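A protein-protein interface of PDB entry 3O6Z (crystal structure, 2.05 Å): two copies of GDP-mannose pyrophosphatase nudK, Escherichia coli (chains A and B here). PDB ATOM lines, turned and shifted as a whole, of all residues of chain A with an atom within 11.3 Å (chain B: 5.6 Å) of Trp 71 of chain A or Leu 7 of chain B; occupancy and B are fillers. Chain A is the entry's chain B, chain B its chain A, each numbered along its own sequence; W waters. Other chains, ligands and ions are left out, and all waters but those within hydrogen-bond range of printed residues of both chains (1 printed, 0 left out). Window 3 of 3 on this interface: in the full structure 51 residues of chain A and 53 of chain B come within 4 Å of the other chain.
No position is printed for both chains.
Of the 6 pairs that touch across the chains among the printed residues, none has its exchanged pair printed and touching as well.
The indole nitrogen (NE1) of Trp 71 of chain A lies close to the backbone carbonyl oxygen (O) of Glu 76 of chain A (3.4 Å).
Of the printed residues of chain B, Trp 71 of chain A touches Leu 7 (3.97 Å).
Leu 7 of chain B touches just one residue of chain A: Trp 71 (3.97 Å).
Of the printed residues of chain A, Ile 5 of chain B touches Phe 66.
No residue of chain A comes within 4 Å of Thr 6 of chain B.
Ile 8 of chain B touches none of the printed residues of chain A.
Of chain A, only Val 68 (3.8 Å) and Val 72 (3.96 Å) come within 4 Å of Ile 23 of chain B.
No residue of chain A comes within 4 Å of Thr 24 of chain B.
Of the printed residues of chain A, Tyr 25 of chain B touches Phe 66 (3.5 Å) and Val 68 (3.7 Å).
Of the printed residues of chain B, Val 72 of chain A touches Ile 23 (3.96 Å).
Printed residues of chain B within 4 Å of Val 68 of chain A: Ile 23 (3.8 Å) and Tyr 25 (3.7 Å).
Asn 73 of chain A touches none of the printed residues of chain B.
Ser 77 of chain A touches none of the printed residues of chain B.
Printed residues of chain B that touch a printed residue of chain A: Ile 5, Leu 7, Ile 23 and Tyr 25.
Hydrophobic or aromatic side chains of chain B within 4 Å of the printed part of chain A: Ile 5, Leu 7, Ile 23 and Tyr 25.
Along chain B the printed residues that touch a printed residue of chain A span positions 5 to 25.
Of the 20 printed residues of chain A, 4 touch a printed residue of chain B.
Among the printed residues, no Asp or Glu carboxylate lies within 4 Å of a Lys or Arg side-chain nitrogen of the other chain.
Ile 5 of chain B touches Phe 66 of chain A (CG2 to CZ, 3.7 Å).
CD2 of Phe 66 of chain A touches CE1 of Tyr 25 of chain B, at 3.5 Å.
CG2 of Val 68 of chain A touches CG2 of Ile 23 of chain B, at 3.8 Å.
CB of Val 68 of chain A touches CE2 of Tyr 25 of chain B (3.7 Å).
Trp 71 of chain A touches Leu 7 of chain B (CH2 to CB, 3.97 Å).
Ile 23 of chain B touches Val 72 of chain A.
Water W1 lies within hydrogen-bond range of OH of Tyr 25 of chain B, O of Phe 66 of chain A and N of Val 68 of chain A.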
ATOM      1  N   ARG A  64     -14.832   2.133  14.806  1.00  0.00           N
ATOM      2  CA  ARG A  64     -14.128   1.537  13.706  1.00  0.00           C
ATOM      3  C   ARG A  64     -15.172   1.198  12.642  1.00  0.00           C
ATOM      4  O   ARG A  64     -16.204   0.575  12.937  1.00  0.00           O
ATOM      5  CB  ARG A  64     -13.364   0.297  14.176  1.00  0.00           C
ATOM      6  CG  ARG A  64     -12.645  -0.479  13.081  1.00  0.00           C
ATOM      7  CD  ARG A  64     -11.827  -1.616  13.723  1.00  0.00           C
ATOM      8  NE  ARG A  64     -10.862  -2.220  12.807  1.00  0.00           N
ATOM      9  CZ  ARG A  64     -10.929  -3.480  12.368  1.00  0.00           C
ATOM     10  NH1 ARG A  64     -11.936  -4.275  12.730  1.00  0.00           N
ATOM     11  NH2 ARG A  64      -9.998  -3.951  11.563  1.00  0.00           N
ATOM     12  N   GLN A  65     -14.913   1.645  11.423  1.00  0.00           N
ATOM     13  CA  GLN A  65     -15.785   1.351  10.277  1.00  0.00           C
ATOM     14  C   GLN A  65     -14.937   1.329   9.017  1.00  0.00           C
ATOM     15  O   GLN A  65     -13.806   1.834   9.012  1.00  0.00           O
ATOM     16  CB  GLN A  65     -16.895   2.410  10.154  1.00  0.00           C
ATOM     17  CG  GLN A  65     -16.433   3.743   9.602  1.00  0.00           C
ATOM     18  CD  GLN A  65     -17.357   4.864   9.975  1.00  0.00           C
ATOM     19  OE1 GLN A  65     -18.479   4.941   9.494  1.00  0.00           O
ATOM     20  NE2 GLN A  65     -16.889   5.749  10.843  1.00  0.00           N
ATOM     21  N   PHE A  66     -15.512   0.756   7.956  1.00  0.00           N
ATOM     22  CA  PHE A  66     -14.888   0.675   6.644  1.00  0.00           C
ATOM     23  C   PHE A  66     -14.922   2.038   6.007  1.00  0.00           C
ATOM     24  O   PHE A  66     -15.983   2.661   5.919  1.00  0.00           O
ATOM     25  CB  PHE A  66     -15.642  -0.320   5.744  1.00  0.00           C
ATOM     26  CG  PHE A  66     -15.023  -0.496   4.404  1.00  0.00           C
ATOM     27  CD1 PHE A  66     -13.783  -1.102   4.283  1.00  0.00           C
ATOM     28  CD2 PHE A  66     -15.657  -0.046   3.263  1.00  0.00           C
ATOM     29  CE1 PHE A  66     -13.200  -1.264   3.026  1.00  0.00           C
ATOM     30  CE2 PHE A  66     -15.067  -0.199   1.990  1.00  0.00           C
ATOM     31  CZ  PHE A  66     -13.857  -0.793   1.874  1.00  0.00           C
ATOM     32  N   ARG A  67     -13.740   2.496   5.606  1.00  0.00           N
ATOM     33  CA  ARG A  67     -13.535   3.753   4.862  1.00  0.00           C
ATOM     34  C   ARG A  67     -12.903   3.427   3.518  1.00  0.00           C
ATOM     35  O   ARG A  67     -11.701   3.174   3.427  1.00  0.00           O
ATOM     36  CB  ARG A  67     -12.603   4.702   5.621  1.00  0.00           C
ATOM     37  CG  ARG A  67     -13.146   5.298   6.918  1.00  0.00           C
ATOM     38  CD  ARG A  67     -14.481   6.100   6.732  1.00  0.00           C
ATOM     39  NE  ARG A  67     -14.690   6.997   7.874  1.00  0.00           N
ATOM     40  CZ  ARG A  67     -15.678   7.868   7.999  1.00  0.00           C
ATOM     41  NH1 ARG A  67     -16.600   7.972   7.050  1.00  0.00           N
ATOM     42  NH2 ARG A  67     -15.735   8.643   9.076  1.00  0.00           N
ATOM     43  N   VAL A  68     -13.723   3.424   2.477  1.00  0.00           N
ATOM     44  CA  VAL A  68     -13.307   3.015   1.133  1.00  0.00           C
ATOM     45  C   VAL A  68     -12.152   3.905   0.579  1.00  0.00           C
ATOM     46  O   VAL A  68     -11.292   3.433  -0.147  1.00  0.00           O
ATOM     47  CB  VAL A  68     -14.545   3.003   0.189  1.00  0.00           C
ATOM     48  CG1 VAL A  68     -15.137   4.422   0.060  1.00  0.00           C
ATOM     49  CG2 VAL A  68     -14.218   2.406  -1.174  1.00  0.00           C
ATOM     50  N   ALA A  69     -12.159   5.181   0.959  1.00  0.00           N
ATOM     51  CA  ALA A  69     -11.115   6.133   0.606  1.00  0.00           C
ATOM     52  C   ALA A  69      -9.737   5.749   1.156  1.00  0.00           C
ATOM     53  O   ALA A  69      -8.732   6.025   0.518  1.00  0.00           O
ATOM     54  CB  ALA A  69     -11.508   7.542   1.088  1.00  0.00           C
ATOM     55  N   THR A  70      -9.686   5.127   2.339  1.00  0.00           N
ATOM     56  CA  THR A  70      -8.403   4.560   2.869  1.00  0.00           C
ATOM     57  C   THR A  70      -8.049   3.187   2.264  1.00  0.00           C
ATOM     58  O   THR A  70      -6.861   2.854   2.055  1.00  0.00           O
ATOM     59  CB  THR A  70      -8.373   4.476   4.414  1.00  0.00           C
ATOM     60  OG1 THR A  70      -9.209   3.403   4.884  1.00  0.00           O
ATOM     61  CG2 THR A  70      -8.765   5.803   5.073  1.00  0.00           C
ATOM     62  N   TRP A  71      -9.089   2.409   1.962  1.00  0.00           N
ATOM     63  CA  TRP A  71      -8.981   1.087   1.341  1.00  0.00           C
ATOM     64  C   TRP A  71      -8.215   1.132   0.032  1.00  0.00           C
ATOM     65  O   TRP A  71      -7.427   0.230  -0.285  1.00  0.00           O
ATOM     66  CB  TRP A  71     -10.392   0.512   1.102  1.00  0.00           C
ATOM     67  CG  TRP A  71     -10.470  -0.960   0.718  1.00  0.00           C
ATOM     68  CD1 TRP A  71      -9.866  -2.009   1.344  1.00  0.00           C
ATOM     69  CD2 TRP A  71     -11.245  -1.522  -0.351  1.00  0.00           C
ATOM     70  NE1 TRP A  71     -10.213  -3.197   0.733  1.00  0.00           N
ATOM     71  CE2 TRP A  71     -11.053  -2.922  -0.317  1.00  0.00           C
ATOM     72  CE3 TRP A  71     -12.077  -0.970  -1.341  1.00  0.00           C
ATOM     73  CZ2 TRP A  71     -11.671  -3.791  -1.241  1.00  0.00           C
ATOM     74  CZ3 TRP A  71     -12.703  -1.831  -2.255  1.00  0.00           C
ATOM     75  CH2 TRP A  71     -12.485  -3.225  -2.204  1.00  0.00           C
ATOM     76  N   VAL A  72      -8.469   2.185  -0.743  1.00  0.00           N
ATOM     77  CA  VAL A  72      -7.883   2.320  -2.073  1.00  0.00           C
ATOM     78  C   VAL A  72      -6.493   2.967  -2.010  1.00  0.00           C
ATOM     79  O   VAL A  72      -5.847   3.166  -3.034  1.00  0.00           O
ATOM     80  CB  VAL A  72      -8.821   3.084  -3.050  1.00  0.00           C
ATOM     81  CG1 VAL A  72     -10.183   2.380  -3.159  1.00  0.00           C
ATOM     82  CG2 VAL A  72      -8.994   4.546  -2.623  1.00  0.00           C
ATOM     83  N   ASN A  73      -6.031   3.231  -0.793  1.00  0.00           N
ATOM     84  CA  ASN A  73      -4.791   3.959  -0.555  1.00  0.00           C
ATOM     85  C   ASN A  73      -4.008   3.488   0.682  1.00  0.00           C
ATOM     86  O   ASN A  73      -3.782   4.266   1.604  1.00  0.00           O
ATOM     87  CB  ASN A  73      -5.089   5.469  -0.475  1.00  0.00           C
ATOM     88  CG  ASN A  73      -3.828   6.315  -0.352  1.00  0.00           C
ATOM     89  OD1 ASN A  73      -2.775   5.976  -0.915  1.00  0.00           O
ATOM     90  ND2 ASN A  73      -3.917   7.403   0.416  1.00  0.00           N
ATOM     91  N   GLY A  74      -3.593   2.218   0.701  1.00  0.00           N
ATOM     92  CA  GLY A  74      -2.694   1.718   1.764  1.00  0.00           C
ATOM     93  C   GLY A  74      -3.286   0.963   2.944  1.00  0.00           C
ATOM     94  O   GLY A  74      -2.595   0.182   3.611  1.00  0.00           O
ATOM     95  N   ASN A  75      -4.570   1.183   3.213  1.00  0.00           N
ATOM     96  CA  ASN A  75      -5.220   0.555   4.341  1.00  0.00           C
ATOM     97  C   ASN A  75      -5.852  -0.765   3.902  1.00  0.00           C
ATOM     98  O   ASN A  75      -6.980  -0.797   3.408  1.00  0.00           O
ATOM     99  CB  ASN A  75      -6.282   1.490   4.912  1.00  0.00           C
ATOM    100  CG  ASN A  75      -6.734   1.097   6.284  1.00  0.00           C
ATOM    101  OD1 ASN A  75      -6.004   0.458   7.065  1.00  0.00           O
ATOM    102  ND2 ASN A  75      -7.942   1.491   6.607  1.00  0.00           N
ATOM    103  N   GLU A  76      -5.109  -1.848   4.116  1.00  0.00           N
ATOM    104  CA  GLU A  76      -5.440  -3.153   3.568  1.00  0.00           C
ATOM    105  C   GLU A  76      -6.895  -3.555   3.746  1.00  0.00           C
ATOM    106  O   GLU A  76      -7.587  -3.873   2.762  1.00  0.00           O
ATOM    107  CB  GLU A  76      -4.494  -4.222   4.130  1.00  0.00           C
ATOM    108  CG  GLU A  76      -4.824  -5.651   3.713  1.00  0.00           C
ATOM    109  CD  GLU A  76      -4.111  -6.086   2.459  1.00  0.00           C
ATOM    110  OE1 GLU A  76      -4.083  -5.308   1.480  1.00  0.00           O
ATOM    111  OE2 GLU A  76      -3.577  -7.218   2.448  1.00  0.00           O
ATOM    112  N   SER A  77      -7.362  -3.542   4.988  1.00  0.00           N
ATOM    113  CA  SER A  77      -8.727  -3.939   5.249  1.00  0.00           C
ATOM    114  C   SER A  77      -9.748  -2.832   4.967  1.00  0.00           C
ATOM    115  O   SER A  77     -10.937  -3.132   4.820  1.00  0.00           O
ATOM    116  CB  SER A  77      -8.885  -4.437   6.690  1.00  0.00           C
ATOM    117  OG  SER A  77      -8.796  -3.334   7.567  1.00  0.00           O
ATOM    118  N   GLY A  78      -9.296  -1.571   4.931  1.00  0.00           N
ATOM    119  CA  GLY A  78     -10.186  -0.406   4.853  1.00  0.00           C
ATOM    120  C   GLY A  78     -10.815   0.009   6.171  1.00  0.00           C
ATOM    121  O   GLY A  78     -11.441   1.081   6.279  1.00  0.00           O
ATOM    122  N   GLN A  79     -10.644  -0.828   7.196  1.00  0.00           N
ATOM    123  CA  GLN A  79     -11.125  -0.509   8.532  1.00  0.00           C
ATOM    124  C   GLN A  79     -10.267   0.550   9.180  1.00  0.00           C
ATOM    125  O   GLN A  79      -9.040   0.515   9.089  1.00  0.00           O
ATOM    126  CB  GLN A  79     -11.206  -1.742   9.415  1.00  0.00           C
ATOM    127  CG  GLN A  79     -12.101  -2.842   8.864  1.00  0.00           C
ATOM    128  CD  GLN A  79     -13.585  -2.505   8.984  1.00  0.00           C
ATOM    129  OE1 GLN A  79     -14.001  -1.795   9.908  1.00  0.00           O
ATOM    130  NE2 GLN A  79     -14.402  -3.066   8.075  1.00  0.00           N
ATOM    131  N   LEU A  80     -10.926   1.537   9.764  1.00  0.00           N
ATOM    132  CA  LEU A  80     -10.227   2.711  10.300  1.00  0.00           C
ATOM    133  C   LEU A  80     -10.805   3.019  11.646  1.00  0.00           C
ATOM    134  O   LEU A  80     -12.034   3.073  11.811  1.00  0.00           O
ATOM    135  CB  LEU A  80     -10.365   3.927   9.354  1.00  0.00           C
ATOM    136  CG  LEU A  80      -9.362   5.065   9.651  1.00  0.00           C
ATOM    137  CD1 LEU A  80      -7.945   4.702   9.213  1.00  0.00           C
ATOM    138  CD2 LEU A  80      -9.791   6.377   9.015  1.00  0.00           C
ATOM    139  N   ILE A  81      -9.914   3.177  12.613  1.00  0.00           N
ATOM    140  CA  ILE A  81     -10.289   3.531  13.970  1.00  0.00           C
ATOM    141  C   ILE A  81     -10.298   5.050  14.022  1.00  0.00           C
ATOM    142  O   ILE A  81      -9.315   5.690  13.626  1.00  0.00           O
ATOM    143  CB  ILE A  81      -9.298   2.987  14.990  1.00  0.00           C
ATOM    144  CG1 ILE A  81      -9.399   1.448  15.072  1.00  0.00           C
ATOM    145  CG2 ILE A  81      -9.511   3.648  16.372  1.00  0.00           C
ATOM    146  CD1 ILE A  81      -8.219   0.813  15.841  1.00  0.00           C
ATOM    147  N   GLU A  82     -11.429   5.621  14.442  1.00  0.00           N
ATOM    148  CA  GLU A  82     -11.552   7.080  14.494  1.00  0.00           C
ATOM    149  C   GLU A  82     -12.333   7.469  15.715  1.00  0.00           C
ATOM    150  O   GLU A  82     -13.016   6.640  16.339  1.00  0.00           O
ATOM    151  CB  GLU A  82     -12.316   7.615  13.279  1.00  0.00           C
ATOM    152  CG  GLU A  82     -11.752   7.283  11.899  1.00  0.00           C
ATOM    153  CD  GLU A  82     -12.802   7.532  10.829  1.00  0.00           C
ATOM    154  OE1 GLU A  82     -13.330   8.658  10.788  1.00  0.00           O
ATOM    155  OE2 GLU A  82     -13.145   6.595  10.072  1.00  0.00           O
ATOM    156  N   ARG A 173      -4.353   5.835  12.808  1.00  0.00           N
ATOM    157  CA  ARG A 173      -3.682   6.547  11.735  1.00  0.00           C
ATOM    158  C   ARG A 173      -4.627   7.567  11.075  1.00  0.00           C
ATOM    159  O   ARG A 173      -4.578   7.792   9.872  1.00  0.00           O
ATOM    160  CB  ARG A 173      -3.084   5.540  10.725  1.00  0.00           C
ATOM    161  CG  ARG A 173      -4.110   4.673   9.991  1.00  0.00           C
ATOM    162  CD  ARG A 173      -3.484   3.810   8.897  1.00  0.00           C
ATOM    163  NE  ARG A 173      -2.760   2.686   9.465  1.00  0.00           N
ATOM    164  CZ  ARG A 173      -2.051   1.793   8.779  1.00  0.00           C
ATOM    165  NH1 ARG A 173      -1.949   1.876   7.465  1.00  0.00           N
ATOM    166  NH2 ARG A 173      -1.422   0.814   9.431  1.00  0.00           N
ATOM    167  N   ILE B   5     -16.186  -7.208   2.277  1.00  0.00           N
ATOM    168  CA  ILE B   5     -16.302  -6.142   1.289  1.00  0.00           C
ATOM    169  C   ILE B   5     -16.121  -6.700  -0.122  1.00  0.00           C
ATOM    170  O   ILE B   5     -15.111  -7.317  -0.425  1.00  0.00           O
ATOM    171  CB  ILE B   5     -15.259  -5.012   1.505  1.00  0.00           C
ATOM    172  CG1 ILE B   5     -15.192  -4.574   2.988  1.00  0.00           C
ATOM    173  CG2 ILE B   5     -15.506  -3.830   0.502  1.00  0.00           C
ATOM    174  CD1 ILE B   5     -16.429  -3.900   3.544  1.00  0.00           C
ATOM    175  N   THR B   6     -17.103  -6.463  -0.982  1.00  0.00           N
ATOM    176  CA  THR B   6     -17.004  -6.853  -2.393  1.00  0.00           C
ATOM    177  C   THR B   6     -17.213  -5.607  -3.233  1.00  0.00           C
ATOM    178  O   THR B   6     -18.291  -5.013  -3.220  1.00  0.00           O
ATOM    179  CB  THR B   6     -18.010  -7.952  -2.773  1.00  0.00           C
ATOM    180  OG1 THR B   6     -17.965  -9.011  -1.802  1.00  0.00           O
ATOM    181  CG2 THR B   6     -17.705  -8.529  -4.179  1.00  0.00           C
ATOM    182  N   LEU B   7     -16.150  -5.203  -3.932  1.00  0.00           N
ATOM    183  CA  LEU B   7     -16.221  -4.090  -4.870  1.00  0.00           C
ATOM    184  C   LEU B   7     -17.158  -4.467  -6.017  1.00  0.00           C
ATOM    185  O   LEU B   7     -17.089  -5.569  -6.531  1.00  0.00           O
ATOM    186  CB  LEU B   7     -14.815  -3.727  -5.383  1.00  0.00           C
ATOM    187  CG  LEU B   7     -14.640  -2.712  -6.517  1.00  0.00           C
ATOM    188  CD1 LEU B   7     -15.080  -1.307  -6.074  1.00  0.00           C
ATOM    189  CD2 LEU B   7     -13.179  -2.696  -6.988  1.00  0.00           C
ATOM    190  N   ILE B   8     -18.047  -3.545  -6.371  1.00  0.00           N
ATOM    191  CA  ILE B   8     -19.091  -3.756  -7.372  1.00  0.00           C
ATOM    192  C   ILE B   8     -18.812  -2.901  -8.614  1.00  0.00           C
ATOM    193  O   ILE B   8     -18.885  -3.380  -9.751  1.00  0.00           O
ATOM    194  CB  ILE B   8     -20.519  -3.421  -6.792  1.00  0.00           C
ATOM    195  CG1 ILE B   8     -20.908  -4.369  -5.632  1.00  0.00           C
ATOM    196  CG2 ILE B   8     -21.602  -3.379  -7.899  1.00  0.00           C
ATOM    197  CD1 ILE B   8     -21.175  -5.814  -6.024  1.00  0.00           C
ATOM    198  N   LYS B   9     -18.505  -1.629  -8.397  1.00  0.00           N
ATOM    199  CA  LYS B   9     -18.284  -0.723  -9.508  1.00  0.00           C
ATOM    200  C   LYS B   9     -17.364   0.389  -9.040  1.00  0.00           C
ATOM    201  O   LYS B   9     -17.367   0.739  -7.856  1.00  0.00           O
ATOM    202  CB  LYS B   9     -19.619  -0.146 -10.019  1.00  0.00           C
ATOM    203  CG  LYS B   9     -19.488   0.817 -11.198  1.00  0.00           C
ATOM    204  CD  LYS B   9     -20.797   1.018 -11.946  1.00  0.00           C
ATOM    205  CE  LYS B   9     -20.695   2.159 -12.980  1.00  0.00           C
ATOM    206  NZ  LYS B   9     -19.663   1.955 -14.068  1.00  0.00           N
ATOM    207  N   ASP B  10     -16.565   0.902  -9.977  1.00  0.00           N
ATOM    208  CA  ASP B  10     -15.789   2.128  -9.779  1.00  0.00           C
ATOM    209  C   ASP B  10     -15.983   3.027 -11.008  1.00  0.00           C
ATOM    210  O   ASP B  10     -15.422   2.769 -12.098  1.00  0.00           O
ATOM    211  CB  ASP B  10     -14.306   1.814  -9.537  1.00  0.00           C
ATOM    212  CG  ASP B  10     -13.466   3.066  -9.257  1.00  0.00           C
ATOM    213  OD1 ASP B  10     -13.985   4.190  -9.364  1.00  0.00           O
ATOM    214  OD2 ASP B  10     -12.269   2.922  -8.922  1.00  0.00           O
ATOM    215  N   ILE B  23     -17.538   4.907  -5.934  1.00  0.00           N
ATOM    216  CA  ILE B  23     -17.235   3.474  -5.694  1.00  0.00           C
ATOM    217  C   ILE B  23     -18.426   2.773  -5.053  1.00  0.00           C
ATOM    218  O   ILE B  23     -18.948   3.230  -4.036  1.00  0.00           O
ATOM    219  CB  ILE B  23     -15.951   3.280  -4.829  1.00  0.00           C
ATOM    220  CG1 ILE B  23     -14.764   3.999  -5.499  1.00  0.00           C
ATOM    221  CG2 ILE B  23     -15.610   1.787  -4.655  1.00  0.00           C
ATOM    222  CD1 ILE B  23     -13.474   3.903  -4.746  1.00  0.00           C
ATOM    223  N   THR B  24     -18.867   1.684  -5.681  1.00  0.00           N
ATOM    224  CA  THR B  24     -19.991   0.904  -5.159  1.00  0.00           C
ATOM    225  C   THR B  24     -19.406  -0.389  -4.657  1.00  0.00           C
ATOM    226  O   THR B  24     -18.629  -1.042  -5.358  1.00  0.00           O
ATOM    227  CB  THR B  24     -21.044   0.610  -6.250  1.00  0.00           C
ATOM    228  OG1 THR B  24     -21.543   1.840  -6.788  1.00  0.00           O
ATOM    229  CG2 THR B  24     -22.193  -0.226  -5.709  1.00  0.00           C
ATOM    230  N   TYR B  25     -19.747  -0.745  -3.425  1.00  0.00           N
ATOM    231  CA  TYR B  25     -19.287  -2.009  -2.845  1.00  0.00           C
ATOM    232  C   TYR B  25     -20.367  -2.555  -1.937  1.00  0.00           C
ATOM    233  O   TYR B  25     -21.154  -1.796  -1.375  1.00  0.00           O
ATOM    234  CB  TYR B  25     -17.976  -1.824  -2.065  1.00  0.00           C
ATOM    235  CG  TYR B  25     -18.072  -0.810  -0.954  1.00  0.00           C
ATOM    236  CD1 TYR B  25     -18.448  -1.195   0.334  1.00  0.00           C
ATOM    237  CD2 TYR B  25     -17.776   0.521  -1.182  1.00  0.00           C
ATOM    238  CE1 TYR B  25     -18.540  -0.285   1.349  1.00  0.00           C
ATOM    239  CE2 TYR B  25     -17.871   1.452  -0.167  1.00  0.00           C
ATOM    240  CZ  TYR B  25     -18.248   1.052   1.088  1.00  0.00           C
ATOM    241  OH  TYR B  25     -18.354   1.975   2.099  1.00  0.00           O
ATOM    242  N   ASP B  26     -20.398  -3.877  -1.813  1.00  0.00           N
ATOM    243  CA  ASP B  26     -21.292  -4.547  -0.897  1.00  0.00           C
ATOM    244  C   ASP B  26     -20.557  -4.806   0.410  1.00  0.00           C
ATOM    245  O   ASP B  26     -19.412  -5.314   0.435  1.00  0.00           O
ATOM    246  CB  ASP B  26     -21.790  -5.888  -1.464  1.00  0.00           C
ATOM    247  CG  ASP B  26     -22.939  -5.731  -2.451  1.00  0.00           C
ATOM    248  OD1 ASP B  26     -23.589  -4.652  -2.491  1.00  0.00           O
ATOM    249  OD2 ASP B  26     -23.210  -6.723  -3.177  1.00  0.00           O
HETATM  250  O   HOH W   1     -16.639   3.675   3.202  1.00  0.00           O
